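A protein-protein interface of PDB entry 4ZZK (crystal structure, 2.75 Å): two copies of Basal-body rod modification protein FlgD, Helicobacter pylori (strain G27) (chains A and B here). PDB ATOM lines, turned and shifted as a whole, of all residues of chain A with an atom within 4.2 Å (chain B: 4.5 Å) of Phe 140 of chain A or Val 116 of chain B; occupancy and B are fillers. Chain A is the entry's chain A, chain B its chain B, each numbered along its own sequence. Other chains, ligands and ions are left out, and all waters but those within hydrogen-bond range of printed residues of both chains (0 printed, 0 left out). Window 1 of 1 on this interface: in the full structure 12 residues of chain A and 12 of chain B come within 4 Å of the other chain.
The side-chain carboxylate of Glu 139 of chain A is in hydrogen-bond range of the side-chain hydroxyl of Ser 115 of chain B (3.2 Å). The backbone carbonyl oxygen (O) of Val 116 of chain B is in hydrogen-bond range of the backbone NH (N) of Phe 140 of chain A (2.8 Å).
No position is printed for both chains. Of the 10 pairs that touch across the chains among the printed residues, none has its exchanged pair printed and touching as well.
Phe 140 of chain A touches five residues of chain B. Val 116 of chain B touches two residues of chain A. Of the printed residues of chain A, Ile 6 of chain B touches Phe 140 (3.6 Å). Of the printed residues of chain B, Ala 137 of chain A touches Phe 118. Met 124 of chain B touches none of the printed residues of chain A. The nearest printed residue of chain B that does not touch Phe 140 of chain A is Ile 117 of chain B (5.0 Å). The nearest printed residue of chain A that does not touch Val 116 of chain B is Tyr 141 of chain A (5.1 Å). The nearest printed residue of chain B that does not touch Tyr 141 of chain A is Ile 6 of chain B (4.1 Å).
Among the printed residues, pairs that only touch across the chains: Phe 140 of chain A with Ser 115 of chain B, Glu 139 of chain A with Val 116 of chain B, Phe 140 of chain A with Val 3 of chain B, Phe 140 of chain A with Ile 6 of chain B, Phe 140 of chain A with Phe 118 of chain B, Glu 139 of chain A with Ile 117 of chain B, Tyr 141 of chain A with Ser 115 of chain B and Ala 137 of chain A with Phe 118 of chain B.
Hydrophobic or aromatic side chains of chain A that line the printed part of chain B: Phe 140 and Tyr 141. Of the 8 printed residues of chain B, 6 touch a printed residue of chain A. Along chain B the printed residues that touch a printed residue of chain A span positions 3 to 118. Among the printed residues, no Asp or Glu carboxylate lies within 4 Å of a Lys or Arg side-chain nitrogen of the other chain.
O of Tyr 141 of chain A lies within hydrogen-bond range of N of Ile 9 of chain A (2.8 Å). The backbone carbonyl oxygen of Ile 117 of chain B is in hydrogen-bond range of the backbone NH of Met 124 of chain B, at 2.8 Å.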
ATOM      1  N   MET A   5      -9.388 -20.060  -3.908  1.00  0.00           N
ATOM      2  CA  MET A   5     -10.535 -20.797  -4.404  1.00  0.00           C
ATOM      3  C   MET A   5     -11.827 -20.444  -3.713  1.00  0.00           C
ATOM      4  O   MET A   5     -12.902 -20.700  -4.255  1.00  0.00           O
ATOM      5  CB  MET A   5     -10.283 -22.282  -4.277  1.00  0.00           C
ATOM      6  CG  MET A   5      -9.146 -22.727  -5.184  1.00  0.00           C
ATOM      7  SD  MET A   5      -8.185 -24.059  -4.480  1.00  0.00           S
ATOM      8  CE  MET A   5      -7.076 -24.460  -5.830  1.00  0.00           C
ATOM      9  N   ILE A   9     -16.758 -20.881  -8.026  1.00  0.00           N
ATOM     10  CA  ILE A   9     -17.412 -22.131  -8.369  1.00  0.00           C
ATOM     11  C   ILE A   9     -16.308 -23.059  -8.809  1.00  0.00           C
ATOM     12  O   ILE A   9     -15.467 -22.660  -9.590  1.00  0.00           O
ATOM     13  CB  ILE A   9     -18.424 -21.965  -9.519  1.00  0.00           C
ATOM     14  CG1 ILE A   9     -19.477 -20.884  -9.193  1.00  0.00           C
ATOM     15  CG2 ILE A   9     -19.130 -23.280  -9.818  1.00  0.00           C
ATOM     16  CD1 ILE A   9     -20.230 -21.080  -7.894  1.00  0.00           C
ATOM     17  N   ALA A  10     -16.324 -24.294  -8.313  1.00  0.00           N
ATOM     18  CA  ALA A  10     -15.361 -25.319  -8.720  1.00  0.00           C
ATOM     19  C   ALA A  10     -16.038 -26.449  -9.469  1.00  0.00           C
ATOM     20  O   ALA A  10     -17.163 -26.848  -9.135  1.00  0.00           O
ATOM     21  CB  ALA A  10     -14.652 -25.879  -7.515  1.00  0.00           C
ATOM     22  N   ALA A 137     -10.150 -30.947  -8.354  1.00  0.00           N
ATOM     23  CA  ALA A 137     -10.722 -29.792  -9.023  1.00  0.00           C
ATOM     24  C   ALA A 137     -10.099 -29.621 -10.374  1.00  0.00           C
ATOM     25  O   ALA A 137      -8.873 -29.592 -10.499  1.00  0.00           O
ATOM     26  CB  ALA A 137     -10.513 -28.542  -8.201  1.00  0.00           C
ATOM     27  N   GLU A 139     -11.617 -27.201 -12.741  1.00  0.00           N
ATOM     28  CA  GLU A 139     -11.891 -25.861 -13.244  1.00  0.00           C
ATOM     29  C   GLU A 139     -12.429 -24.955 -12.138  1.00  0.00           C
ATOM     30  O   GLU A 139     -13.195 -25.400 -11.288  1.00  0.00           O
ATOM     31  CB  GLU A 139     -12.894 -25.918 -14.401  1.00  0.00           C
ATOM     32  CG  GLU A 139     -13.092 -24.604 -15.138  1.00  0.00           C
ATOM     33  CD  GLU A 139     -13.975 -24.725 -16.367  1.00  0.00           C
ATOM     34  OE1 GLU A 139     -14.728 -25.716 -16.488  1.00  0.00           O
ATOM     35  OE2 GLU A 139     -13.938 -23.791 -17.204  1.00  0.00           O
ATOM     36  N   PHE A 140     -12.034 -23.677 -12.184  1.00  0.00           N
ATOM     37  CA  PHE A 140     -12.624 -22.649 -11.337  1.00  0.00           C
ATOM     38  C   PHE A 140     -13.087 -21.449 -12.160  1.00  0.00           C
ATOM     39  O   PHE A 140     -12.452 -21.101 -13.164  1.00  0.00           O
ATOM     40  CB  PHE A 140     -11.610 -22.172 -10.310  1.00  0.00           C
ATOM     41  CG  PHE A 140     -11.142 -23.239  -9.363  1.00  0.00           C
ATOM     42  CD1 PHE A 140     -10.057 -24.039  -9.678  1.00  0.00           C
ATOM     43  CD2 PHE A 140     -11.796 -23.433  -8.146  1.00  0.00           C
ATOM     44  CE1 PHE A 140      -9.622 -25.027  -8.806  1.00  0.00           C
ATOM     45  CE2 PHE A 140     -11.397 -24.424  -7.278  1.00  0.00           C
ATOM     46  CZ  PHE A 140     -10.291 -25.219  -7.598  1.00  0.00           C
ATOM     47  N   TYR A 141     -14.170 -20.816 -11.718  1.00  0.00           N
ATOM     48  CA  TYR A 141     -14.651 -19.539 -12.274  1.00  0.00           C
ATOM     49  C   TYR A 141     -15.528 -18.797 -11.270  1.00  0.00           C
ATOM     50  O   TYR A 141     -15.943 -19.389 -10.284  1.00  0.00           O
ATOM     51  CB  TYR A 141     -15.433 -19.758 -13.581  1.00  0.00           C
ATOM     52  CG  TYR A 141     -16.494 -20.845 -13.552  1.00  0.00           C
ATOM     53  CD1 TYR A 141     -17.781 -20.568 -13.141  1.00  0.00           C
ATOM     54  CD2 TYR A 141     -16.191 -22.162 -13.928  1.00  0.00           C
ATOM     55  CE1 TYR A 141     -18.753 -21.550 -13.083  1.00  0.00           C
ATOM     56  CE2 TYR A 141     -17.160 -23.146 -13.885  1.00  0.00           C
ATOM     57  CZ  TYR A 141     -18.446 -22.828 -13.464  1.00  0.00           C
ATOM     58  OH  TYR A 141     -19.405 -23.787 -13.403  1.00  0.00           O
ATOM     59  N   VAL B   3      -5.315 -19.572  -8.396  1.00  0.00           N
ATOM     60  CA  VAL B   3      -6.583 -19.212  -9.013  1.00  0.00           C
ATOM     61  C   VAL B   3      -6.861 -17.701  -8.843  1.00  0.00           C
ATOM     62  O   VAL B   3      -7.852 -17.144  -9.321  1.00  0.00           O
ATOM     63  CB  VAL B   3      -7.670 -20.086  -8.325  1.00  0.00           C
ATOM     64  CG1 VAL B   3      -9.069 -19.494  -8.376  1.00  0.00           C
ATOM     65  CG2 VAL B   3      -7.656 -21.479  -8.925  1.00  0.00           C
ATOM     66  N   ILE B   6      -8.052 -15.111 -11.673  1.00  0.00           N
ATOM     67  CA  ILE B   6      -9.397 -14.954 -12.160  1.00  0.00           C
ATOM     68  C   ILE B   6      -9.881 -13.570 -11.814  1.00  0.00           C
ATOM     69  O   ILE B   6      -9.765 -13.143 -10.683  1.00  0.00           O
ATOM     70  CB  ILE B   6     -10.360 -15.994 -11.560  1.00  0.00           C
ATOM     71  CG1 ILE B   6      -9.860 -17.424 -11.877  1.00  0.00           C
ATOM     72  CG2 ILE B   6     -11.756 -15.805 -12.125  1.00  0.00           C
ATOM     73  CD1 ILE B   6     -10.727 -18.544 -11.323  1.00  0.00           C
ATOM     74  N   SER B 115     -11.761 -17.933 -16.353  1.00  0.00           N
ATOM     75  CA  SER B 115     -11.705 -19.140 -15.572  1.00  0.00           C
ATOM     76  C   SER B 115     -10.298 -19.726 -15.620  1.00  0.00           C
ATOM     77  O   SER B 115      -9.487 -19.315 -16.424  1.00  0.00           O
ATOM     78  CB  SER B 115     -12.754 -20.153 -16.084  1.00  0.00           C
ATOM     79  OG  SER B 115     -12.221 -21.094 -17.012  1.00  0.00           O
ATOM     80  N   VAL B 116     -10.005 -20.634 -14.693  1.00  0.00           N
ATOM     81  CA  VAL B 116      -8.752 -21.391 -14.687  1.00  0.00           C
ATOM     82  C   VAL B 116      -9.112 -22.853 -14.785  1.00  0.00           C
ATOM     83  O   VAL B 116     -10.005 -23.309 -14.078  1.00  0.00           O
ATOM     84  CB  VAL B 116      -7.916 -21.187 -13.405  1.00  0.00           C
ATOM     85  CG1 VAL B 116      -6.701 -22.107 -13.386  1.00  0.00           C
ATOM     86  CG2 VAL B 116      -7.447 -19.756 -13.320  1.00  0.00           C
ATOM     87  N   ILE B 117      -8.417 -23.565 -15.664  1.00  0.00           N
ATOM     88  CA  ILE B 117      -8.745 -24.950 -15.999  1.00  0.00           C
ATOM     89  C   ILE B 117      -7.529 -25.798 -15.727  1.00  0.00           C
ATOM     90  O   ILE B 117      -6.463 -25.483 -16.220  1.00  0.00           O
ATOM     91  CB  ILE B 117      -9.097 -25.103 -17.487  1.00  0.00           C
ATOM     92  CG1 ILE B 117     -10.365 -24.322 -17.797  1.00  0.00           C
ATOM     93  CG2 ILE B 117      -9.273 -26.577 -17.862  1.00  0.00           C
ATOM     94  CD1 ILE B 117     -10.513 -24.027 -19.267  1.00  0.00           C
ATOM     95  N   PHE B 118      -7.697 -26.863 -14.954  1.00  0.00           N
ATOM     96  CA  PHE B 118      -6.623 -27.834 -14.729  1.00  0.00           C
ATOM     97  C   PHE B 118      -6.760 -29.005 -15.687  1.00  0.00           C
ATOM     98  O   PHE B 118      -7.686 -29.833 -15.561  1.00  0.00           O
ATOM     99  CB  PHE B 118      -6.597 -28.278 -13.273  1.00  0.00           C
ATOM    100  CG  PHE B 118      -6.210 -27.169 -12.343  1.00  0.00           C
ATOM    101  CD1 PHE B 118      -7.156 -26.245 -11.906  1.00  0.00           C
ATOM    102  CD2 PHE B 118      -4.896 -26.997 -11.960  1.00  0.00           C
ATOM    103  CE1 PHE B 118      -6.804 -25.198 -11.066  1.00  0.00           C
ATOM    104  CE2 PHE B 118      -4.536 -25.946 -11.124  1.00  0.00           C
ATOM    105  CZ  PHE B 118      -5.490 -25.041 -10.682  1.00  0.00           C
ATOM    106  N   MET B 124      -4.331 -23.784 -16.905  1.00  0.00           N
ATOM    107  CA  MET B 124      -4.650 -23.089 -18.160  1.00  0.00           C
ATOM    108  C   MET B 124      -5.626 -21.913 -17.912  1.00  0.00           C
ATOM    109  O   MET B 124      -6.516 -22.013 -17.073  1.00  0.00           O
ATOM    110  CB  MET B 124      -5.331 -24.060 -19.138  1.00  0.00           C
ATOM    111  CG  MET B 124      -4.627 -25.386 -19.396  1.00  0.00           C
ATOM    112  SD  MET B 124      -3.177 -25.239 -20.463  1.00  0.00           S
ATOM    113  CE  MET B 124      -3.973 -24.981 -22.053  1.00  0.00           C
ATOM    114  N   LEU B 125      -5.473 -20.834 -18.666  1.00  0.00           N
ATOM    115  CA  LEU B 125      -6.295 -19.658 -18.485  1.00  0.00           C
ATOM    116  C   LEU B 125      -7.289 -19.563 -19.601  1.00  0.00           C
ATOM    117  O   LEU B 125      -6.898 -19.563 -20.747  1.00  0.00           O
ATOM    118  CB  LEU B 125      -5.443 -18.381 -18.516  1.00  0.00           C
ATOM    119  CG  LEU B 125      -4.299 -18.308 -17.536  1.00  0.00           C
ATOM    120  CD1 LEU B 125      -3.506 -17.026 -17.743  1.00  0.00           C
ATOM    121  CD2 LEU B 125      -4.833 -18.374 -16.118  1.00  0.00           C
